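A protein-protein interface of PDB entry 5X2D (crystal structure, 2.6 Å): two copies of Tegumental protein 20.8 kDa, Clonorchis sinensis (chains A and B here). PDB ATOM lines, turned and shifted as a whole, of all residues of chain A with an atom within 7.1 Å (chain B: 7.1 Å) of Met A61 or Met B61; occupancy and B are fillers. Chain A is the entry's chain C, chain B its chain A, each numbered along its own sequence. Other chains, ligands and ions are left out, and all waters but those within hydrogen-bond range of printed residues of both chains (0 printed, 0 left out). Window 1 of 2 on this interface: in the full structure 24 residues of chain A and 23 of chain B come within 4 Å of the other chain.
O of Thr A70 is in hydrogen-bond range of NE2 of Gln B59.
O of Val B60 lies within hydrogen-bond range of N of Thr A70 (3.1 Å).
The backbone NH of Trp A68 is in hydrogen-bond range of the backbone carbonyl oxygen of Val B62 (2.9 Å).
N of Trp B68 lies within hydrogen-bond range of O of Val A62 (2.9 Å).
The backbone NH (N) of Thr B70 is in hydrogen-bond range of the backbone carbonyl oxygen (O) of Val A60 (3.1 Å).
Of chain B, only Met B61, Trp B68 and Ile B69 come within 4 Å of Met A61.
Met B61 touches three residues of chain A.
Of the printed residues of chain A, Ile B69 touches Gln A59 (3.3 Å), Val A60 (3.5 Å) and Met A61 (3.6 Å).
Printed residues of chain B within 4 Å of Val A60: Trp B68 (3.6 Å), Ile B69 (3.5 Å) and Thr B70 (3.1 Å).
Printed residues of chain B within 4 Å of Gln A59: Ile B69 (3.3 Å) and Thr B70 (3.5 Å).
Printed residues of chain B within 4 Å of Val A62: Tyr B67 and Trp B68.
Printed residues of chain B within 4 Å of Trp A91: Trp B91.
Ala B87 touches none of the printed residues of chain A.
Leu A89 touches none of the printed residues of chain B.
The nearest residue of chain B that does not touch Met A61 is Tyr B67 (4.7 Å).
The nearest printed residue of chain B that does not touch Ile A69 is Thr B43 (4.2 Å).
Thr A43 touches Thr B70, and with the chains exchanged Thr A70 touches Thr B43.
Val A60 touches Trp B68, and with the chains exchanged Trp A68 touches Val B60.
Met A61 touches its own counterpart, Met B61.
Met A61 touches Trp B68, and with the chains exchanged Trp A68 touches Met B61.
Positions printed for both chains: 43, 59, 60, 61, 62, 63, 67, 68, 69, 70, 80, 87, 88, 89, 90 and 91.
Of the 25 pairs that touch across the chains among the printed residues, 24 have their exchanged pair printed and touching as well.
Trp B68 touches Thr A43 (O to CG2, 3.5 Å).
Thr A43 touches Thr B70.
Gln A59 touches Thr B70.
O of Trp B68 touches O of Val A60, at 3.6 Å.
Val A60 touches Ile B69.
O of Val A62 touches CA of Tyr B67, at 3.2 Å.
Tyr A67 touches Val B62 (CA to O, 3.1 Å).
Val B60 touches Trp A68 (O to O, 3.5 Å).
Thr A70 touches Thr B43.
CH2 of Trp A91 touches CH2 of Trp B91, at 3.8 Å.
Hydrophobic or aromatic side chains of chain A that line the printed part of chain B: Val A60, Met A61, Tyr A67, Trp A68, Ile A69 and Trp A91.
Of the 16 printed residues of chain B, 11 touch a printed residue of chain A.
The backbone NH of Gln B59 sits at hydrogen-bond distance from the backbone carbonyl oxygen of Trp B91, at 2.6 Å.
The backbone carbonyl oxygen (O) of Met B61 sits at hydrogen-bond distance from the backbone NH (N) of Leu B89.
The side-chain amide oxygen (OE1) of Gln B80 sits at hydrogen-bond distance from the side-chain hydroxyl (OH) of Tyr B67 (2.9 Å).
N of Gln A59 sits at hydrogen-bond distance from O of Trp A91, at 2.7 Å.
The backbone NH of Leu A89 is in hydrogen-bond range of the backbone carbonyl oxygen of Met A61, at 2.7 Å.
OE1 of Gln A80 sits at hydrogen-bond distance from OH of Tyr A67 (2.8 Å).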
ATOM      1  N   THR A  43      17.018  29.704 -35.476  1.00  0.00           N
ATOM      2  CA  THR A  43      18.130  28.815 -35.740  1.00  0.00           C
ATOM      3  C   THR A  43      18.193  28.611 -37.236  1.00  0.00           C
ATOM      4  O   THR A  43      19.250  28.727 -37.840  1.00  0.00           O
ATOM      5  CB  THR A  43      17.976  27.451 -35.046  1.00  0.00           C
ATOM      6  OG1 THR A  43      16.810  26.797 -35.541  1.00  0.00           O
ATOM      7  CG2 THR A  43      17.851  27.617 -33.545  1.00  0.00           C
ATOM      8  N   GLN A  59      25.039  23.313 -38.686  1.00  0.00           N
ATOM      9  CA  GLN A  59      24.072  23.018 -37.647  1.00  0.00           C
ATOM     10  C   GLN A  59      24.150  24.050 -36.546  1.00  0.00           C
ATOM     11  O   GLN A  59      25.210  24.256 -35.964  1.00  0.00           O
ATOM     12  CB  GLN A  59      24.266  21.634 -37.042  1.00  0.00           C
ATOM     13  CG  GLN A  59      22.968  21.207 -36.383  1.00  0.00           C
ATOM     14  CD  GLN A  59      22.921  19.762 -35.974  1.00  0.00           C
ATOM     15  OE1 GLN A  59      23.899  19.219 -35.440  1.00  0.00           O
ATOM     16  NE2 GLN A  59      21.771  19.122 -36.207  1.00  0.00           N
ATOM     17  N   VAL A  60      23.033  24.712 -36.272  1.00  0.00           N
ATOM     18  CA  VAL A  60      22.989  25.768 -35.263  1.00  0.00           C
ATOM     19  C   VAL A  60      22.134  25.322 -34.078  1.00  0.00           C
ATOM     20  O   VAL A  60      20.968  24.939 -34.246  1.00  0.00           O
ATOM     21  CB  VAL A  60      22.439  27.087 -35.839  1.00  0.00           C
ATOM     22  CG1 VAL A  60      22.288  28.127 -34.738  1.00  0.00           C
ATOM     23  CG2 VAL A  60      23.347  27.601 -36.936  1.00  0.00           C
ATOM     24  N   MET A  61      22.730  25.301 -32.892  1.00  0.00           N
ATOM     25  CA  MET A  61      21.981  24.934 -31.699  1.00  0.00           C
ATOM     26  C   MET A  61      21.931  26.074 -30.686  1.00  0.00           C
ATOM     27  O   MET A  61      22.970  26.606 -30.310  1.00  0.00           O
ATOM     28  CB  MET A  61      22.575  23.692 -31.041  1.00  0.00           C
ATOM     29  CG  MET A  61      21.909  23.388 -29.718  1.00  0.00           C
ATOM     30  SD  MET A  61      22.444  21.833 -29.022  1.00  0.00           S
ATOM     31  CE  MET A  61      24.186  22.121 -29.000  1.00  0.00           C
ATOM     32  N   VAL A  62      20.727  26.436 -30.242  1.00  0.00           N
ATOM     33  CA  VAL A  62      20.541  27.481 -29.216  1.00  0.00           C
ATOM     34  C   VAL A  62      20.154  26.881 -27.860  1.00  0.00           C
ATOM     35  O   VAL A  62      19.290  26.019 -27.791  1.00  0.00           O
ATOM     36  CB  VAL A  62      19.455  28.510 -29.631  1.00  0.00           C
ATOM     37  CG1 VAL A  62      19.329  29.611 -28.603  1.00  0.00           C
ATOM     38  CG2 VAL A  62      19.752  29.091 -31.008  1.00  0.00           C
ATOM     39  N   VAL A  63      20.797  27.329 -26.786  1.00  0.00           N
ATOM     40  CA  VAL A  63      20.509  26.789 -25.451  1.00  0.00           C
ATOM     41  C   VAL A  63      20.121  27.868 -24.437  1.00  0.00           C
ATOM     42  O   VAL A  63      20.785  28.910 -24.343  1.00  0.00           O
ATOM     43  CB  VAL A  63      21.723  26.013 -24.864  1.00  0.00           C
ATOM     44  CG1 VAL A  63      21.412  25.506 -23.455  1.00  0.00           C
ATOM     45  CG2 VAL A  63      22.099  24.880 -25.734  1.00  0.00           C
ATOM     46  N   TYR A  67      25.397  23.662 -19.882  1.00  0.00           N
ATOM     47  CA  TYR A  67      25.638  22.365 -20.523  1.00  0.00           C
ATOM     48  C   TYR A  67      27.060  21.833 -20.405  1.00  0.00           C
ATOM     49  O   TYR A  67      27.987  22.572 -20.114  1.00  0.00           O
ATOM     50  CB  TYR A  67      25.241  22.446 -21.993  1.00  0.00           C
ATOM     51  CG  TYR A  67      26.112  23.318 -22.866  1.00  0.00           C
ATOM     52  CD1 TYR A  67      27.302  22.820 -23.416  1.00  0.00           C
ATOM     53  CD2 TYR A  67      25.728  24.614 -23.197  1.00  0.00           C
ATOM     54  CE1 TYR A  67      28.092  23.594 -24.235  1.00  0.00           C
ATOM     55  CE2 TYR A  67      26.515  25.400 -24.023  1.00  0.00           C
ATOM     56  CZ  TYR A  67      27.696  24.875 -24.539  1.00  0.00           C
ATOM     57  OH  TYR A  67      28.497  25.623 -25.356  1.00  0.00           O
ATOM     58  N   TRP A  68      27.203  20.528 -20.614  1.00  0.00           N
ATOM     59  CA  TRP A  68      28.492  19.849 -20.523  1.00  0.00           C
ATOM     60  C   TRP A  68      28.749  18.887 -21.690  1.00  0.00           C
ATOM     61  O   TRP A  68      28.080  17.866 -21.790  1.00  0.00           O
ATOM     62  CB  TRP A  68      28.563  19.071 -19.192  1.00  0.00           C
ATOM     63  CG  TRP A  68      28.601  19.928 -17.966  1.00  0.00           C
ATOM     64  CD1 TRP A  68      29.705  20.293 -17.270  1.00  0.00           C
ATOM     65  CD2 TRP A  68      27.490  20.522 -17.293  1.00  0.00           C
ATOM     66  NE1 TRP A  68      29.358  21.088 -16.207  1.00  0.00           N
ATOM     67  CE2 TRP A  68      27.996  21.245 -16.200  1.00  0.00           C
ATOM     68  CE3 TRP A  68      26.105  20.516 -17.506  1.00  0.00           C
ATOM     69  CZ2 TRP A  68      27.179  21.949 -15.320  1.00  0.00           C
ATOM     70  CZ3 TRP A  68      25.288  21.228 -16.632  1.00  0.00           C
ATOM     71  CH2 TRP A  68      25.826  21.929 -15.556  1.00  0.00           C
ATOM     72  N   ILE A  69      29.740  19.173 -22.538  1.00  0.00           N
ATOM     73  CA  ILE A  69      30.058  18.265 -23.656  1.00  0.00           C
ATOM     74  C   ILE A  69      31.339  17.487 -23.444  1.00  0.00           C
ATOM     75  O   ILE A  69      32.323  18.051 -23.004  1.00  0.00           O
ATOM     76  CB  ILE A  69      30.209  19.008 -25.001  1.00  0.00           C
ATOM     77  CG1 ILE A  69      29.083  20.017 -25.210  1.00  0.00           C
ATOM     78  CG2 ILE A  69      30.204  18.013 -26.170  1.00  0.00           C
ATOM     79  CD1 ILE A  69      28.925  20.447 -26.675  1.00  0.00           C
ATOM     80  N   THR A  70      31.341  16.202 -23.802  1.00  0.00           N
ATOM     81  CA  THR A  70      32.590  15.454 -23.793  1.00  0.00           C
ATOM     82  C   THR A  70      33.481  16.107 -24.808  1.00  0.00           C
ATOM     83  O   THR A  70      33.004  16.725 -25.751  1.00  0.00           O
ATOM     84  CB  THR A  70      32.434  13.972 -24.173  1.00  0.00           C
ATOM     85  OG1 THR A  70      31.919  13.861 -25.502  1.00  0.00           O
ATOM     86  CG2 THR A  70      31.507  13.282 -23.233  1.00  0.00           C
ATOM     87  N   GLN A  80      31.243  28.945 -30.411  1.00  0.00           N
ATOM     88  CA  GLN A  80      30.287  28.841 -29.321  1.00  0.00           C
ATOM     89  C   GLN A  80      30.351  30.105 -28.466  1.00  0.00           C
ATOM     90  O   GLN A  80      31.385  30.417 -27.904  1.00  0.00           O
ATOM     91  CB  GLN A  80      30.547  27.577 -28.494  1.00  0.00           C
ATOM     92  CG  GLN A  80      30.423  26.280 -29.300  1.00  0.00           C
ATOM     93  CD  GLN A  80      30.498  25.038 -28.439  1.00  0.00           C
ATOM     94  OE1 GLN A  80      30.500  25.127 -27.219  1.00  0.00           O
ATOM     95  NE2 GLN A  80      30.609  23.874 -29.071  1.00  0.00           N
ATOM     96  N   ALA A  87      23.071  30.785 -25.131  1.00  0.00           N
ATOM     97  CA  ALA A  87      24.197  30.211 -25.883  1.00  0.00           C
ATOM     98  C   ALA A  87      23.830  29.858 -27.310  1.00  0.00           C
ATOM     99  O   ALA A  87      22.715  29.409 -27.597  1.00  0.00           O
ATOM    100  CB  ALA A  87      24.745  28.956 -25.181  1.00  0.00           C
ATOM    101  N   TYR A  88      24.808  30.035 -28.189  1.00  0.00           N
ATOM    102  CA  TYR A  88      24.693  29.712 -29.596  1.00  0.00           C
ATOM    103  C   TYR A  88      25.834  28.795 -30.017  1.00  0.00           C
ATOM    104  O   TYR A  88      27.005  29.139 -29.855  1.00  0.00           O
ATOM    105  CB  TYR A  88      24.678  31.000 -30.428  1.00  0.00           C
ATOM    106  CG  TYR A  88      23.460  31.842 -30.133  1.00  0.00           C
ATOM    107  CD1 TYR A  88      23.444  32.719 -29.059  1.00  0.00           C
ATOM    108  CD2 TYR A  88      22.303  31.733 -30.912  1.00  0.00           C
ATOM    109  CE1 TYR A  88      22.322  33.474 -28.766  1.00  0.00           C
ATOM    110  CE2 TYR A  88      21.171  32.493 -30.626  1.00  0.00           C
ATOM    111  CZ  TYR A  88      21.188  33.362 -29.550  1.00  0.00           C
ATOM    112  OH  TYR A  88      20.079  34.125 -29.241  1.00  0.00           O
ATOM    113  N   LEU A  89      25.499  27.624 -30.544  1.00  0.00           N
ATOM    114  CA  LEU A  89      26.507  26.682 -31.026  1.00  0.00           C
ATOM    115  C   LEU A  89      26.447  26.559 -32.554  1.00  0.00           C
ATOM    116  O   LEU A  89      25.391  26.253 -33.131  1.00  0.00           O
ATOM    117  CB  LEU A  89      26.326  25.302 -30.369  1.00  0.00           C
ATOM    118  CG  LEU A  89      26.787  25.190 -28.915  1.00  0.00           C
ATOM    119  CD1 LEU A  89      25.700  25.670 -27.985  1.00  0.00           C
ATOM    120  CD2 LEU A  89      27.206  23.776 -28.554  1.00  0.00           C
ATOM    121  N   PHE A  90      27.578  26.800 -33.208  1.00  0.00           N
ATOM    122  CA  PHE A  90      27.671  26.622 -34.650  1.00  0.00           C
ATOM    123  C   PHE A  90      28.611  25.484 -34.994  1.00  0.00           C
ATOM    124  O   PHE A  90      29.717  25.395 -34.447  1.00  0.00           O
ATOM    125  CB  PHE A  90      28.137  27.904 -35.324  1.00  0.00           C
ATOM    126  CG  PHE A  90      27.135  29.018 -35.253  1.00  0.00           C
ATOM    127  CD1 PHE A  90      26.849  29.647 -34.038  1.00  0.00           C
ATOM    128  CD2 PHE A  90      26.510  29.480 -36.400  1.00  0.00           C
ATOM    129  CE1 PHE A  90      25.932  30.696 -33.966  1.00  0.00           C
ATOM    130  CE2 PHE A  90      25.590  30.535 -36.337  1.00  0.00           C
ATOM    131  CZ  PHE A  90      25.306  31.143 -35.115  1.00  0.00           C
ATOM    132  N   TRP A  91      28.156  24.622 -35.904  1.00  0.00           N
ATOM    133  CA  TRP A  91      28.960  23.545 -36.473  1.00  0.00           C
ATOM    134  C   TRP A  91      28.798  23.547 -37.958  1.00  0.00           C
ATOM    135  O   TRP A  91      27.687  23.399 -38.446  1.00  0.00           O
ATOM    136  CB  TRP A  91      28.520  22.161 -35.986  1.00  0.00           C
ATOM    137  CG  TRP A  91      28.705  21.865 -34.557  1.00  0.00           C
ATOM    138  CD1 TRP A  91      29.888  21.804 -33.875  1.00  0.00           C
ATOM    139  CD2 TRP A  91      27.678  21.535 -33.618  1.00  0.00           C
ATOM    140  NE1 TRP A  91      29.656  21.473 -32.558  1.00  0.00           N
ATOM    141  CE2 TRP A  91      28.307  21.303 -32.374  1.00  0.00           C
ATOM    142  CE3 TRP A  91      26.287  21.417 -33.702  1.00  0.00           C
ATOM    143  CZ2 TRP A  91      27.593  20.964 -31.229  1.00  0.00           C
ATOM    144  CZ3 TRP A  91      25.583  21.082 -32.565  1.00  0.00           C
ATOM    145  CH2 TRP A  91      26.239  20.857 -31.345  1.00  0.00           C
ATOM    146  N   THR B  43      29.759  13.086 -18.320  1.00  0.00           N
ATOM    147  CA  THR B  43      29.598  12.965 -19.746  1.00  0.00           C
ATOM    148  C   THR B  43      30.672  12.002 -20.195  1.00  0.00           C
ATOM    149  O   THR B  43      30.388  11.039 -20.892  1.00  0.00           O
ATOM    150  CB  THR B  43      29.748  14.313 -20.466  1.00  0.00           C
ATOM    151  OG1 THR B  43      31.066  14.828 -20.242  1.00  0.00           O
ATOM    152  CG2 THR B  43      28.726  15.306 -19.961  1.00  0.00           C
ATOM    153  N   GLN B  59      29.795  11.568 -28.936  1.00  0.00           N
ATOM    154  CA  GLN B  59      29.795  12.845 -28.243  1.00  0.00           C
ATOM    155  C   GLN B  59      28.546  12.950 -27.394  1.00  0.00           C
ATOM    156  O   GLN B  59      27.425  12.847 -27.903  1.00  0.00           O
ATOM    157  CB  GLN B  59      29.893  14.027 -29.205  1.00  0.00           C
ATOM    158  CG  GLN B  59      30.435  15.246 -28.474  1.00  0.00           C
ATOM    159  CD  GLN B  59      30.856  16.372 -29.378  1.00  0.00           C
ATOM    160  OE1 GLN B  59      30.264  16.583 -30.442  1.00  0.00           O
ATOM    161  NE2 GLN B  59      31.895  17.111 -28.963  1.00  0.00           N
ATOM    162  N   VAL B  60      28.749  13.135 -26.089  1.00  0.00           N
ATOM    163  CA  VAL B  60      27.650  13.161 -25.129  1.00  0.00           C
ATOM    164  C   VAL B  60      27.497  14.576 -24.591  1.00  0.00           C
ATOM    165  O   VAL B  60      28.432  15.152 -24.021  1.00  0.00           O
ATOM    166  CB  VAL B  60      27.882  12.187 -23.953  1.00  0.00           C
ATOM    167  CG1 VAL B  60      26.753  12.294 -22.946  1.00  0.00           C
ATOM    168  CG2 VAL B  60      27.987  10.772 -24.447  1.00  0.00           C
ATOM    169  N   MET B  61      26.327  15.154 -24.805  1.00  0.00           N
ATOM    170  CA  MET B  61      26.077  16.490 -24.305  1.00  0.00           C
ATOM    171  C   MET B  61      24.937  16.463 -23.301  1.00  0.00           C
ATOM    172  O   MET B  61      23.868  15.924 -23.583  1.00  0.00           O
ATOM    173  CB  MET B  61      25.765  17.444 -25.452  1.00  0.00           C
ATOM    174  CG  MET B  61      25.332  18.812 -24.987  1.00  0.00           C
ATOM    175  SD  MET B  61      25.186  19.908 -26.392  1.00  0.00           S
ATOM    176  CE  MET B  61      24.077  18.976 -27.392  1.00  0.00           C
ATOM    177  N   VAL B  62      25.182  17.010 -22.118  1.00  0.00           N
ATOM    178  CA  VAL B  62      24.161  17.103 -21.084  1.00  0.00           C
ATOM    179  C   VAL B  62      23.707  18.553 -20.918  1.00  0.00           C
ATOM    180  O   VAL B  62      24.534  19.458 -20.852  1.00  0.00           O
ATOM    181  CB  VAL B  62      24.683  16.555 -19.736  1.00  0.00           C
ATOM    182  CG1 VAL B  62      23.578  16.545 -18.686  1.00  0.00           C
ATOM    183  CG2 VAL B  62      25.277  15.156 -19.926  1.00  0.00           C
ATOM    184  N   VAL B  63      22.397  18.773 -20.861  1.00  0.00           N
ATOM    185  CA  VAL B  63      21.854  20.126 -20.725  1.00  0.00           C
ATOM    186  C   VAL B  63      20.889  20.295 -19.554  1.00  0.00           C
ATOM    187  O   VAL B  63      20.025  19.449 -19.312  1.00  0.00           O
ATOM    188  CB  VAL B  63      21.135  20.581 -22.011  1.00  0.00           C
ATOM    189  CG1 VAL B  63      20.495  21.968 -21.821  1.00  0.00           C
ATOM    190  CG2 VAL B  63      22.096  20.597 -23.148  1.00  0.00           C
ATOM    191  N   TYR B  67      16.303  23.858 -25.333  1.00  0.00           N
ATOM    192  CA  TYR B  67      17.147  24.073 -26.516  1.00  0.00           C
ATOM    193  C   TYR B  67      16.456  23.932 -27.868  1.00  0.00           C
ATOM    194  O   TYR B  67      15.320  23.451 -27.958  1.00  0.00           O
ATOM    195  CB  TYR B  67      18.367  23.155 -26.459  1.00  0.00           C
ATOM    196  CG  TYR B  67      18.119  21.674 -26.607  1.00  0.00           C
ATOM    197  CD1 TYR B  67      17.979  21.094 -27.865  1.00  0.00           C
ATOM    198  CD2 TYR B  67      18.128  20.839 -25.500  1.00  0.00           C
ATOM    199  CE1 TYR B  67      17.797  19.746 -28.003  1.00  0.00           C
ATOM    200  CE2 TYR B  67      17.938  19.482 -25.628  1.00  0.00           C
ATOM    201  CZ  TYR B  67      17.780  18.943 -26.886  1.00  0.00           C
ATOM    202  OH  TYR B  67      17.587  17.592 -27.047  1.00  0.00           O
ATOM    203  N   TRP B  68      17.115  24.478 -28.891  1.00  0.00           N
ATOM    204  CA  TRP B  68      16.633  24.446 -30.273  1.00  0.00           C
ATOM    205  C   TRP B  68      17.704  24.116 -31.329  1.00  0.00           C
ATOM    206  O   TRP B  68      18.617  24.910 -31.536  1.00  0.00           O
ATOM    207  CB  TRP B  68      15.999  25.802 -30.617  1.00  0.00           C
ATOM    208  CG  TRP B  68      14.721  26.088 -29.870  1.00  0.00           C
ATOM    209  CD1 TRP B  68      13.471  25.896 -30.326  1.00  0.00           C
ATOM    210  CD2 TRP B  68      14.598  26.625 -28.545  1.00  0.00           C
ATOM    211  NE1 TRP B  68      12.552  26.263 -29.370  1.00  0.00           N
ATOM    212  CE2 TRP B  68      13.213  26.714 -28.271  1.00  0.00           C
ATOM    213  CE3 TRP B  68      15.505  27.047 -27.565  1.00  0.00           C
ATOM    214  CZ2 TRP B  68      12.724  27.205 -27.059  1.00  0.00           C
ATOM    215  CZ3 TRP B  68      15.012  27.528 -26.348  1.00  0.00           C
ATOM    216  CH2 TRP B  68      13.634  27.606 -26.113  1.00  0.00           C
ATOM    217  N   ILE B  69      17.594  22.981 -32.020  1.00  0.00           N
ATOM    218  CA  ILE B  69      18.545  22.667 -33.101  1.00  0.00           C
ATOM    219  C   ILE B  69      17.938  22.767 -34.494  1.00  0.00           C
ATOM    220  O   ILE B  69      16.801  22.366 -34.702  1.00  0.00           O
ATOM    221  CB  ILE B  69      19.156  21.257 -32.971  1.00  0.00           C
ATOM    222  CG1 ILE B  69      19.640  20.991 -31.549  1.00  0.00           C
ATOM    223  CG2 ILE B  69      20.355  21.095 -33.926  1.00  0.00           C
ATOM    224  CD1 ILE B  69      20.655  19.833 -31.473  1.00  0.00           C
ATOM    225  N   THR B  70      18.711  23.268 -35.458  1.00  0.00           N
ATOM    226  CA  THR B  70      18.274  23.242 -36.850  1.00  0.00           C
ATOM    227  C   THR B  70      18.126  21.791 -37.259  1.00  0.00           C
ATOM    228  O   THR B  70      18.748  20.910 -36.669  1.00  0.00           O
ATOM    229  CB  THR B  70      19.268  23.915 -37.808  1.00  0.00           C
ATOM    230  OG1 THR B  70      20.502  23.187 -37.820  1.00  0.00           O
ATOM    231  CG2 THR B  70      19.512  25.345 -37.395  1.00  0.00           C
ATOM    232  N   GLN B  80      18.238  11.122 -27.963  1.00  0.00           N
ATOM    233  CA  GLN B  80      18.095  12.328 -27.146  1.00  0.00           C
ATOM    234  C   GLN B  80      16.943  12.168 -26.171  1.00  0.00           C
ATOM    235  O   GLN B  80      15.817  12.032 -26.600  1.00  0.00           O
ATOM    236  CB  GLN B  80      17.885  13.566 -28.028  1.00  0.00           C
ATOM    237  CG  GLN B  80      19.043  13.856 -28.982  1.00  0.00           C
ATOM    238  CD  GLN B  80      18.887  15.164 -29.726  1.00  0.00           C
ATOM    239  OE1 GLN B  80      18.001  15.951 -29.435  1.00  0.00           O
ATOM    240  NE2 GLN B  80      19.708  15.369 -30.739  1.00  0.00           N
ATOM    241  N   ALA B  87      18.427  16.997 -19.917  1.00  0.00           N
ATOM    242  CA  ALA B  87      18.496  16.323 -21.216  1.00  0.00           C
ATOM    243  C   ALA B  87      19.862  15.732 -21.484  1.00  0.00           C
ATOM    244  O   ALA B  87      20.888  16.307 -21.109  1.00  0.00           O
ATOM    245  CB  ALA B  87      18.120  17.281 -22.346  1.00  0.00           C
ATOM    246  N   TYR B  88      19.853  14.596 -22.175  1.00  0.00           N
ATOM    247  CA  TYR B  88      21.063  13.895 -22.561  1.00  0.00           C
ATOM    248  C   TYR B  88      21.073  13.681 -24.065  1.00  0.00           C
ATOM    249  O   TYR B  88      20.146  13.092 -24.624  1.00  0.00           O
ATOM    250  CB  TYR B  88      21.170  12.558 -21.816  1.00  0.00           C
ATOM    251  CG  TYR B  88      21.291  12.735 -20.319  1.00  0.00           C
ATOM    252  CD1 TYR B  88      20.161  12.864 -19.520  1.00  0.00           C
ATOM    253  CD2 TYR B  88      22.543  12.824 -19.705  1.00  0.00           C
ATOM    254  CE1 TYR B  88      20.269  13.046 -18.156  1.00  0.00           C
ATOM    255  CE2 TYR B  88      22.660  13.010 -18.339  1.00  0.00           C
ATOM    256  CZ  TYR B  88      21.518  13.121 -17.568  1.00  0.00           C
ATOM    257  OH  TYR B  88      21.619  13.312 -16.202  1.00  0.00           O
ATOM    258  N   LEU B  89      22.108  14.174 -24.729  1.00  0.00           N
ATOM    259  CA  LEU B  89      22.226  14.003 -26.170  1.00  0.00           C
ATOM    260  C   LEU B  89      23.386  13.062 -26.517  1.00  0.00           C
ATOM    261  O   LEU B  89      24.533  13.280 -26.085  1.00  0.00           O
ATOM    262  CB  LEU B  89      22.416  15.361 -26.869  1.00  0.00           C
ATOM    263  CG  LEU B  89      21.187  16.269 -26.962  1.00  0.00           C
ATOM    264  CD1 LEU B  89      21.081  17.079 -25.707  1.00  0.00           C
ATOM    265  CD2 LEU B  89      21.209  17.176 -28.178  1.00  0.00           C
ATOM    266  N   PHE B  90      23.092  12.011 -27.279  1.00  0.00           N
ATOM    267  CA  PHE B  90      24.142  11.122 -27.765  1.00  0.00           C
ATOM    268  C   PHE B  90      24.274  11.206 -29.279  1.00  0.00           C
ATOM    269  O   PHE B  90      23.267  11.185 -30.000  1.00  0.00           O
ATOM    270  CB  PHE B  90      23.883   9.676 -27.341  1.00  0.00           C
ATOM    271  CG  PHE B  90      23.990   9.459 -25.855  1.00  0.00           C
ATOM    272  CD1 PHE B  90      22.990   9.931 -24.990  1.00  0.00           C
ATOM    273  CD2 PHE B  90      25.092   8.807 -25.309  1.00  0.00           C
ATOM    274  CE1 PHE B  90      23.078   9.734 -23.612  1.00  0.00           C
ATOM    275  CE2 PHE B  90      25.195   8.609 -23.932  1.00  0.00           C
ATOM    276  CZ  PHE B  90      24.183   9.076 -23.079  1.00  0.00           C
ATOM    277  N   TRP B  91      25.523  11.322 -29.734  1.00  0.00           N
ATOM    278  CA  TRP B  91      25.894  11.259 -31.144  1.00  0.00           C
ATOM    279  C   TRP B  91      27.080  10.343 -31.311  1.00  0.00           C
ATOM    280  O   TRP B  91      28.148  10.636 -30.788  1.00  0.00           O
ATOM    281  CB  TRP B  91      26.328  12.617 -31.701  1.00  0.00           C
ATOM    282  CG  TRP B  91      25.323  13.692 -31.780  1.00  0.00           C
ATOM    283  CD1 TRP B  91      24.185  13.702 -32.528  1.00  0.00           C
ATOM    284  CD2 TRP B  91      25.391  14.967 -31.130  1.00  0.00           C
ATOM    285  NE1 TRP B  91      23.525  14.897 -32.368  1.00  0.00           N
ATOM    286  CE2 TRP B  91      24.244  15.691 -31.512  1.00  0.00           C
ATOM    287  CE3 TRP B  91      26.308  15.563 -30.255  1.00  0.00           C
ATOM    288  CZ2 TRP B  91      23.985  16.977 -31.050  1.00  0.00           C
ATOM    289  CZ3 TRP B  91      26.050  16.835 -29.800  1.00  0.00           C
ATOM    290  CH2 TRP B  91      24.901  17.529 -30.205  1.00  0.00           C
